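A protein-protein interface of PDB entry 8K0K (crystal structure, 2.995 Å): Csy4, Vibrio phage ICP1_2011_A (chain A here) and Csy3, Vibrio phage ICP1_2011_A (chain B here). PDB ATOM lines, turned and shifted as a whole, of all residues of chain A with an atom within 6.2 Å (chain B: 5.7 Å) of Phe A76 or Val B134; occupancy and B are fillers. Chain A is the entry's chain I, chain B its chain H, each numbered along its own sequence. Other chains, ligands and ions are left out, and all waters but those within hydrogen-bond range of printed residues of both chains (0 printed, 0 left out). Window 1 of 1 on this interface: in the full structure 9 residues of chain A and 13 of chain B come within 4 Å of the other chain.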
ATOM      1  N   THR A   8      18.419   2.460 -33.979  1.00  0.00           N
ATOM      2  CA  THR A   8      17.266   3.108 -33.370  1.00  0.00           C
ATOM      3  C   THR A   8      17.740   4.049 -32.269  1.00  0.00           C
ATOM      4  O   THR A   8      18.583   3.678 -31.444  1.00  0.00           O
ATOM      5  CB  THR A   8      16.278   2.083 -32.807  1.00  0.00           C
ATOM      6  OG1 THR A   8      16.673   1.704 -31.483  1.00  0.00           O
ATOM      7  CG2 THR A   8      16.240   0.844 -33.687  1.00  0.00           C
ATOM      8  N   VAL A   9      17.206   5.266 -32.270  1.00  0.00           N
ATOM      9  CA  VAL A   9      17.517   6.241 -31.231  1.00  0.00           C
ATOM     10  C   VAL A   9      16.617   5.982 -30.030  1.00  0.00           C
ATOM     11  O   VAL A   9      15.390   5.920 -30.161  1.00  0.00           O
ATOM     12  CB  VAL A   9      17.340   7.671 -31.761  1.00  0.00           C
ATOM     13  CG1 VAL A   9      17.550   8.676 -30.643  1.00  0.00           C
ATOM     14  CG2 VAL A   9      18.296   7.929 -32.916  1.00  0.00           C
ATOM     15  N   VAL A  10      17.225   5.831 -28.855  1.00  0.00           N
ATOM     16  CA  VAL A  10      16.490   5.531 -27.632  1.00  0.00           C
ATOM     17  C   VAL A  10      17.063   6.374 -26.499  1.00  0.00           C
ATOM     18  O   VAL A  10      18.267   6.651 -26.463  1.00  0.00           O
ATOM     19  CB  VAL A  10      16.543   4.022 -27.301  1.00  0.00           C
ATOM     20  CG1 VAL A  10      17.967   3.586 -26.983  1.00  0.00           C
ATOM     21  CG2 VAL A  10      15.588   3.677 -26.163  1.00  0.00           C
ATOM     22  N   ASP A  11      16.184   6.802 -25.587  1.00  0.00           N
ATOM     23  CA  ASP A  11      16.564   7.566 -24.395  1.00  0.00           C
ATOM     24  C   ASP A  11      17.318   8.843 -24.763  1.00  0.00           C
ATOM     25  O   ASP A  11      18.426   9.103 -24.288  1.00  0.00           O
ATOM     26  CB  ASP A  11      17.372   6.701 -23.425  1.00  0.00           C
ATOM     27  CG  ASP A  11      16.501   5.728 -22.654  1.00  0.00           C
ATOM     28  OD1 ASP A  11      15.585   5.136 -23.264  1.00  0.00           O
ATOM     29  OD2 ASP A  11      16.730   5.552 -21.439  1.00  0.00           O
ATOM     30  N   ALA A  12      16.693   9.649 -25.623  1.00  0.00           N
ATOM     31  CA  ALA A  12      17.239  10.939 -26.027  1.00  0.00           C
ATOM     32  C   ALA A  12      16.205  12.055 -25.898  1.00  0.00           C
ATOM     33  O   ALA A  12      16.342  13.101 -26.543  1.00  0.00           O
ATOM     34  CB  ALA A  12      17.779  10.872 -27.457  1.00  0.00           C
ATOM     35  N   ASP A  14      15.831  13.928 -23.398  1.00  0.00           N
ATOM     36  CA  ASP A  14      16.578  15.079 -22.901  1.00  0.00           C
ATOM     37  C   ASP A  14      16.896  16.032 -24.042  1.00  0.00           C
ATOM     38  O   ASP A  14      16.705  17.248 -23.933  1.00  0.00           O
ATOM     39  CB  ASP A  14      17.884  14.632 -22.236  1.00  0.00           C
ATOM     40  CG  ASP A  14      17.691  13.526 -21.222  1.00  0.00           C
ATOM     41  OD1 ASP A  14      17.268  12.416 -21.613  1.00  0.00           O
ATOM     42  OD2 ASP A  14      17.995  13.764 -20.032  1.00  0.00           O
ATOM     43  N   VAL A  15      17.369  15.480 -25.159  1.00  0.00           N
ATOM     44  CA  VAL A  15      17.971  16.236 -26.243  1.00  0.00           C
ATOM     45  C   VAL A  15      17.171  16.122 -27.537  1.00  0.00           C
ATOM     46  O   VAL A  15      17.612  16.608 -28.579  1.00  0.00           O
ATOM     47  CB  VAL A  15      19.435  15.801 -26.454  1.00  0.00           C
ATOM     48  CG1 VAL A  15      20.243  16.899 -27.116  1.00  0.00           C
ATOM     49  CG2 VAL A  15      20.064  15.417 -25.124  1.00  0.00           C
ATOM     50  N   PHE A  19      17.041  15.657 -33.255  1.00  0.00           N
ATOM     51  CA  PHE A  19      18.392  16.202 -33.161  1.00  0.00           C
ATOM     52  C   PHE A  19      19.428  15.086 -33.142  1.00  0.00           C
ATOM     53  O   PHE A  19      20.461  15.172 -33.821  1.00  0.00           O
ATOM     54  CB  PHE A  19      18.529  17.077 -31.919  1.00  0.00           C
ATOM     55  CG  PHE A  19      19.920  17.599 -31.704  1.00  0.00           C
ATOM     56  CD1 PHE A  19      20.503  18.454 -32.626  1.00  0.00           C
ATOM     57  CD2 PHE A  19      20.645  17.236 -30.582  1.00  0.00           C
ATOM     58  CE1 PHE A  19      21.787  18.937 -32.433  1.00  0.00           C
ATOM     59  CE2 PHE A  19      21.929  17.716 -30.381  1.00  0.00           C
ATOM     60  CZ  PHE A  19      22.499  18.568 -31.309  1.00  0.00           C
ATOM     61  N   VAL A  20      19.162  14.022 -32.383  1.00  0.00           N
ATOM     62  CA  VAL A  20      20.068  12.877 -32.378  1.00  0.00           C
ATOM     63  C   VAL A  20      20.156  12.268 -33.769  1.00  0.00           C
ATOM     64  O   VAL A  20      21.250  12.069 -34.295  1.00  0.00           O
ATOM     65  CB  VAL A  20      19.633  11.831 -31.339  1.00  0.00           C
ATOM     66  CG1 VAL A  20      20.425  10.549 -31.544  1.00  0.00           C
ATOM     67  CG2 VAL A  20      19.859  12.365 -29.942  1.00  0.00           C
ATOM     68  N   LYS A  23      22.282  14.147 -35.892  1.00  0.00           N
ATOM     69  CA  LYS A  23      23.683  13.984 -35.505  1.00  0.00           C
ATOM     70  C   LYS A  23      24.239  12.652 -35.997  1.00  0.00           C
ATOM     71  O   LYS A  23      25.392  12.571 -36.435  1.00  0.00           O
ATOM     72  CB  LYS A  23      23.825  14.095 -33.986  1.00  0.00           C
ATOM     73  CG  LYS A  23      25.113  14.765 -33.529  1.00  0.00           C
ATOM     74  CD  LYS A  23      24.919  16.265 -33.364  1.00  0.00           C
ATOM     75  CE  LYS A  23      26.249  16.996 -33.338  1.00  0.00           C
ATOM     76  NZ  LYS A  23      26.947  16.887 -34.647  1.00  0.00           N
ATOM     77  N   VAL A  24      23.420  11.603 -35.951  1.00  0.00           N
ATOM     78  CA  VAL A  24      23.854  10.264 -36.342  1.00  0.00           C
ATOM     79  C   VAL A  24      24.112  10.216 -37.839  1.00  0.00           C
ATOM     80  O   VAL A  24      25.185   9.799 -38.291  1.00  0.00           O
ATOM     81  CB  VAL A  24      22.806   9.213 -35.927  1.00  0.00           C
ATOM     82  CG1 VAL A  24      23.221   7.828 -36.405  1.00  0.00           C
ATOM     83  CG2 VAL A  24      22.594   9.223 -34.422  1.00  0.00           C
ATOM     84  N   THR A  72      30.847   8.220 -30.565  1.00  0.00           N
ATOM     85  CA  THR A  72      30.581   9.480 -29.880  1.00  0.00           C
ATOM     86  C   THR A  72      29.130   9.614 -29.438  1.00  0.00           C
ATOM     87  O   THR A  72      28.842  10.406 -28.532  1.00  0.00           O
ATOM     88  CB  THR A  72      30.948  10.660 -30.784  1.00  0.00           C
ATOM     89  OG1 THR A  72      30.351  10.475 -32.073  1.00  0.00           O
ATOM     90  CG2 THR A  72      32.457  10.764 -30.941  1.00  0.00           C
ATOM     91  N   LEU A  73      28.215   8.864 -30.051  1.00  0.00           N
ATOM     92  CA  LEU A  73      26.794   8.954 -29.739  1.00  0.00           C
ATOM     93  C   LEU A  73      26.221   7.638 -29.231  1.00  0.00           C
ATOM     94  O   LEU A  73      25.006   7.548 -29.010  1.00  0.00           O
ATOM     95  CB  LEU A  73      26.005   9.411 -30.971  1.00  0.00           C
ATOM     96  CG  LEU A  73      26.785  10.018 -32.140  1.00  0.00           C
ATOM     97  CD1 LEU A  73      25.928  10.047 -33.385  1.00  0.00           C
ATOM     98  CD2 LEU A  73      27.265  11.416 -31.823  1.00  0.00           C
ATOM     99  N   THR A  74      27.062   6.623 -29.018  1.00  0.00           N
ATOM    100  CA  THR A  74      26.591   5.275 -28.709  1.00  0.00           C
ATOM    101  C   THR A  74      25.654   5.208 -27.507  1.00  0.00           C
ATOM    102  O   THR A  74      24.987   4.184 -27.328  1.00  0.00           O
ATOM    103  CB  THR A  74      27.785   4.339 -28.477  1.00  0.00           C
ATOM    104  OG1 THR A  74      28.996   5.105 -28.398  1.00  0.00           O
ATOM    105  CG2 THR A  74      27.906   3.318 -29.613  1.00  0.00           C
ATOM    106  N   ASP A  75      25.569   6.262 -26.688  1.00  0.00           N
ATOM    107  CA  ASP A  75      24.698   6.211 -25.518  1.00  0.00           C
ATOM    108  C   ASP A  75      23.239   6.496 -25.845  1.00  0.00           C
ATOM    109  O   ASP A  75      22.364   6.146 -25.045  1.00  0.00           O
ATOM    110  CB  ASP A  75      25.175   7.192 -24.441  1.00  0.00           C
ATOM    111  CG  ASP A  75      26.169   6.565 -23.475  1.00  0.00           C
ATOM    112  OD1 ASP A  75      26.347   5.328 -23.516  1.00  0.00           O
ATOM    113  OD2 ASP A  75      26.773   7.308 -22.672  1.00  0.00           O
ATOM    114  N   PHE A  76      22.955   7.132 -26.986  1.00  0.00           N
ATOM    115  CA  PHE A  76      21.585   7.364 -27.432  1.00  0.00           C
ATOM    116  C   PHE A  76      21.193   6.439 -28.577  1.00  0.00           C
ATOM    117  O   PHE A  76      20.240   6.728 -29.310  1.00  0.00           O
ATOM    118  CB  PHE A  76      21.393   8.820 -27.860  1.00  0.00           C
ATOM    119  CG  PHE A  76      21.877   9.820 -26.857  1.00  0.00           C
ATOM    120  CD1 PHE A  76      21.175  10.039 -25.682  1.00  0.00           C
ATOM    121  CD2 PHE A  76      23.027  10.551 -27.095  1.00  0.00           C
ATOM    122  CE1 PHE A  76      21.618  10.961 -24.761  1.00  0.00           C
ATOM    123  CE2 PHE A  76      23.475  11.475 -26.179  1.00  0.00           C
ATOM    124  CZ  PHE A  76      22.768  11.684 -25.010  1.00  0.00           C
ATOM    125  N   ILE A  77      21.905   5.331 -28.742  1.00  0.00           N
ATOM    126  CA  ILE A  77      21.856   4.543 -29.964  1.00  0.00           C
ATOM    127  C   ILE A  77      21.763   3.066 -29.610  1.00  0.00           C
ATOM    128  O   ILE A  77      22.437   2.589 -28.691  1.00  0.00           O
ATOM    129  CB  ILE A  77      23.090   4.839 -30.842  1.00  0.00           C
ATOM    130  CG1 ILE A  77      22.798   6.005 -31.788  1.00  0.00           C
ATOM    131  CG2 ILE A  77      23.547   3.605 -31.595  1.00  0.00           C
ATOM    132  CD1 ILE A  77      24.017   6.492 -32.531  1.00  0.00           C
ATOM    133  N   HIS A  78      20.912   2.344 -30.339  1.00  0.00           N
ATOM    134  CA  HIS A  78      20.807   0.893 -30.249  1.00  0.00           C
ATOM    135  C   HIS A  78      20.946   0.356 -31.666  1.00  0.00           C
ATOM    136  O   HIS A  78      20.042   0.533 -32.490  1.00  0.00           O
ATOM    137  CB  HIS A  78      19.478   0.472 -29.621  1.00  0.00           C
ATOM    138  CG  HIS A  78      19.340  -1.005 -29.411  1.00  0.00           C
ATOM    139  ND1 HIS A  78      19.436  -1.917 -30.439  1.00  0.00           N
ATOM    140  CD2 HIS A  78      19.088  -1.724 -28.292  1.00  0.00           C
ATOM    141  CE1 HIS A  78      19.264  -3.137 -29.960  1.00  0.00           C
ATOM    142  NE2 HIS A  78      19.049  -3.047 -28.660  1.00  0.00           N
ATOM    143  N   TRP B 130      22.921  19.017 -21.166  1.00  0.00           N
ATOM    144  CA  TRP B 130      21.888  18.853 -22.189  1.00  0.00           C
ATOM    145  C   TRP B 130      22.489  18.626 -23.575  1.00  0.00           C
ATOM    146  O   TRP B 130      23.232  17.661 -23.777  1.00  0.00           O
ATOM    147  CB  TRP B 130      20.948  20.062 -22.203  1.00  0.00           C
ATOM    148  CG  TRP B 130      20.203  20.250 -20.912  1.00  0.00           C
ATOM    149  CD1 TRP B 130      20.518  21.111 -19.900  1.00  0.00           C
ATOM    150  CD2 TRP B 130      19.023  19.554 -20.491  1.00  0.00           C
ATOM    151  NE1 TRP B 130      19.609  20.994 -18.877  1.00  0.00           N
ATOM    152  CE2 TRP B 130      18.680  20.046 -19.216  1.00  0.00           C
ATOM    153  CE3 TRP B 130      18.225  18.564 -21.069  1.00  0.00           C
ATOM    154  CZ2 TRP B 130      17.575  19.583 -18.511  1.00  0.00           C
ATOM    155  CZ3 TRP B 130      17.131  18.103 -20.366  1.00  0.00           C
ATOM    156  CH2 TRP B 130      16.813  18.614 -19.101  1.00  0.00           C
ATOM    157  N   ARG B 131      22.192  19.518 -24.530  1.00  0.00           N
ATOM    158  CA  ARG B 131      22.654  19.354 -25.909  1.00  0.00           C
ATOM    159  C   ARG B 131      24.172  19.366 -26.037  1.00  0.00           C
ATOM    160  O   ARG B 131      24.695  18.944 -27.075  1.00  0.00           O
ATOM    161  CB  ARG B 131      22.086  20.461 -26.809  1.00  0.00           C
ATOM    162  CG  ARG B 131      20.591  20.391 -27.111  1.00  0.00           C
ATOM    163  CD  ARG B 131      20.330  20.376 -28.620  1.00  0.00           C
ATOM    164  NE  ARG B 131      18.984  20.839 -28.958  1.00  0.00           N
ATOM    165  CZ  ARG B 131      17.914  20.053 -29.014  1.00  0.00           C
ATOM    166  NH1 ARG B 131      18.028  18.762 -28.754  1.00  0.00           N
ATOM    167  NH2 ARG B 131      16.727  20.557 -29.325  1.00  0.00           N
ATOM    168  N   ASN B 132      24.893  19.854 -25.028  1.00  0.00           N
ATOM    169  CA  ASN B 132      26.338  19.982 -25.158  1.00  0.00           C
ATOM    170  C   ASN B 132      27.074  18.664 -24.960  1.00  0.00           C
ATOM    171  O   ASN B 132      28.232  18.553 -25.376  1.00  0.00           O
ATOM    172  CB  ASN B 132      26.872  21.024 -24.170  1.00  0.00           C
ATOM    173  CG  ASN B 132      26.349  22.419 -24.455  1.00  0.00           C
ATOM    174  OD1 ASN B 132      26.955  23.184 -25.206  1.00  0.00           O
ATOM    175  ND2 ASN B 132      25.215  22.757 -23.853  1.00  0.00           N
ATOM    176  N   ARG B 133      26.436  17.666 -24.340  1.00  0.00           N
ATOM    177  CA  ARG B 133      27.064  16.361 -24.177  1.00  0.00           C
ATOM    178  C   ARG B 133      26.881  15.465 -25.394  1.00  0.00           C
ATOM    179  O   ARG B 133      27.627  14.490 -25.546  1.00  0.00           O
ATOM    180  CB  ARG B 133      26.507  15.656 -22.937  1.00  0.00           C
ATOM    181  CG  ARG B 133      25.090  15.130 -23.096  1.00  0.00           C
ATOM    182  CD  ARG B 133      24.558  14.598 -21.781  1.00  0.00           C
ATOM    183  NE  ARG B 133      23.140  14.257 -21.847  1.00  0.00           N
ATOM    184  CZ  ARG B 133      22.672  13.015 -21.909  1.00  0.00           C
ATOM    185  NH1 ARG B 133      23.511  11.988 -21.913  1.00  0.00           N
ATOM    186  NH2 ARG B 133      21.363  12.796 -21.964  1.00  0.00           N
ATOM    187  N   VAL B 134      25.917  15.774 -26.262  1.00  0.00           N
ATOM    188  CA  VAL B 134      25.643  14.948 -27.433  1.00  0.00           C
ATOM    189  C   VAL B 134      26.765  15.123 -28.447  1.00  0.00           C
ATOM    190  O   VAL B 134      27.074  16.243 -28.869  1.00  0.00           O
ATOM    191  CB  VAL B 134      24.283  15.303 -28.043  1.00  0.00           C
ATOM    192  CG1 VAL B 134      24.162  14.734 -29.443  1.00  0.00           C
ATOM    193  CG2 VAL B 134      23.169  14.780 -27.163  1.00  0.00           C
ATOM    194  N   GLY B 135      27.380  14.011 -28.842  1.00  0.00           N
ATOM    195  CA  GLY B 135      28.437  14.046 -29.829  1.00  0.00           C
ATOM    196  C   GLY B 135      29.812  14.340 -29.283  1.00  0.00           C
ATOM    197  O   GLY B 135      30.662  14.853 -30.019  1.00  0.00           O
ATOM    198  N   ALA B 136      30.066  14.026 -28.019  1.00  0.00           N
ATOM    199  CA  ALA B 136      31.332  14.344 -27.377  1.00  0.00           C
ATOM    200  C   ALA B 136      32.268  13.145 -27.441  1.00  0.00           C
ATOM    201  O   ALA B 136      31.872  12.024 -27.101  1.00  0.00           O
ATOM    202  CB  ALA B 136      31.113  14.770 -25.927  1.00  0.00           C
ATOM    203  N   ASN B 158      22.016   7.914 -18.153  1.00  0.00           N
ATOM    204  CA  ASN B 158      20.666   7.365 -18.069  1.00  0.00           C
ATOM    205  C   ASN B 158      20.476   6.360 -16.936  1.00  0.00           C
ATOM    206  O   ASN B 158      19.344   5.918 -16.711  1.00  0.00           O
ATOM    207  CB  ASN B 158      20.298   6.727 -19.412  1.00  0.00           C
ATOM    208  CG  ASN B 158      20.306   7.734 -20.553  1.00  0.00           C
ATOM    209  OD1 ASN B 158      19.669   8.787 -20.470  1.00  0.00           O
ATOM    210  ND2 ASN B 158      21.041   7.425 -21.616  1.00  0.00           N
ATOM    211  N   LEU B 193      34.734  18.271 -28.423  1.00  0.00           N
ATOM    212  CA  LEU B 193      33.738  18.453 -29.470  1.00  0.00           C
ATOM    213  C   LEU B 193      34.320  18.757 -30.843  1.00  0.00           C
ATOM    214  O   LEU B 193      33.662  18.474 -31.846  1.00  0.00           O
ATOM    215  CB  LEU B 193      32.763  19.579 -29.086  1.00  0.00           C
ATOM    216  CG  LEU B 193      31.962  19.371 -27.798  1.00  0.00           C
ATOM    217  CD1 LEU B 193      30.988  20.516 -27.581  1.00  0.00           C
ATOM    218  CD2 LEU B 193      31.229  18.039 -27.825  1.00  0.00           C
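CE3 of Trp B130 touches O of Asp A14, 3.5 Å away.
Asp A14 touches Arg B133 (CG to NH2, 3.8 Å).
Arg B131 touches Phe A19.
Val B134 touches Phe A19.
Gly B135 touches Thr A72.
Thr A72 touches Ala B136.
Gly B135 touches Leu A73 (CA to CD2, 3.5 Å).
Asp A75 touches Asn B158 (O to ND2, 3.9 Å).
CZ of Phe A76 touches NH1 of Arg B133, 3.2 Å away.
Val B134 touches Phe A76.
Of the 9 printed residues of chain B, 7 touch a printed residue of chain A.
Hydrophobic or aromatic side chains of chain B within 4 Å of the printed part of chain A: Trp B130 and Val B134.
Hydrophobic or aromatic side chains of chain A that line the printed part of chain B: Val A15, Phe A19, Leu A73 and Phe A76.
Among the printed residues, no Asp or Glu carboxylate lies within 4 Å of a Lys or Arg side-chain nitrogen of the other chain.
The backbone NH (N) of Val A10 sits at hydrogen-bond distance from the backbone carbonyl oxygen (O) of Phe A76, 3.2 Å away.
The backbone carbonyl oxygen (O) of Val A15 sits close to the guanidinium group (NH1) of Arg B131, at 2.2 Å.
Of the printed residues of chain B, Val A15 touches Arg B131 and Val B134.
Of the printed residues of chain B, Thr A72 touches Gly B135 and Ala B136.
Thr A74 touches none of the printed residues of chain B.
Of chain B, only Arg B133 (3.2 Å) and Val B134 (3.5 Å) come within 4 Å of Phe A76.
Of the printed residues of chain A, Trp B130 touches Asp A14.
Printed residues of chain A within 4 Å of Gly B135: Thr A72 (3.9 Å) and Leu A73 (3.5 Å).
The nearest residue of chain B that does not touch Phe A76 is Asn B158 (4.8 Å).
The nearest printed residue of chain B that does not touch Asp A75 is Arg B133 (5.7 Å).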
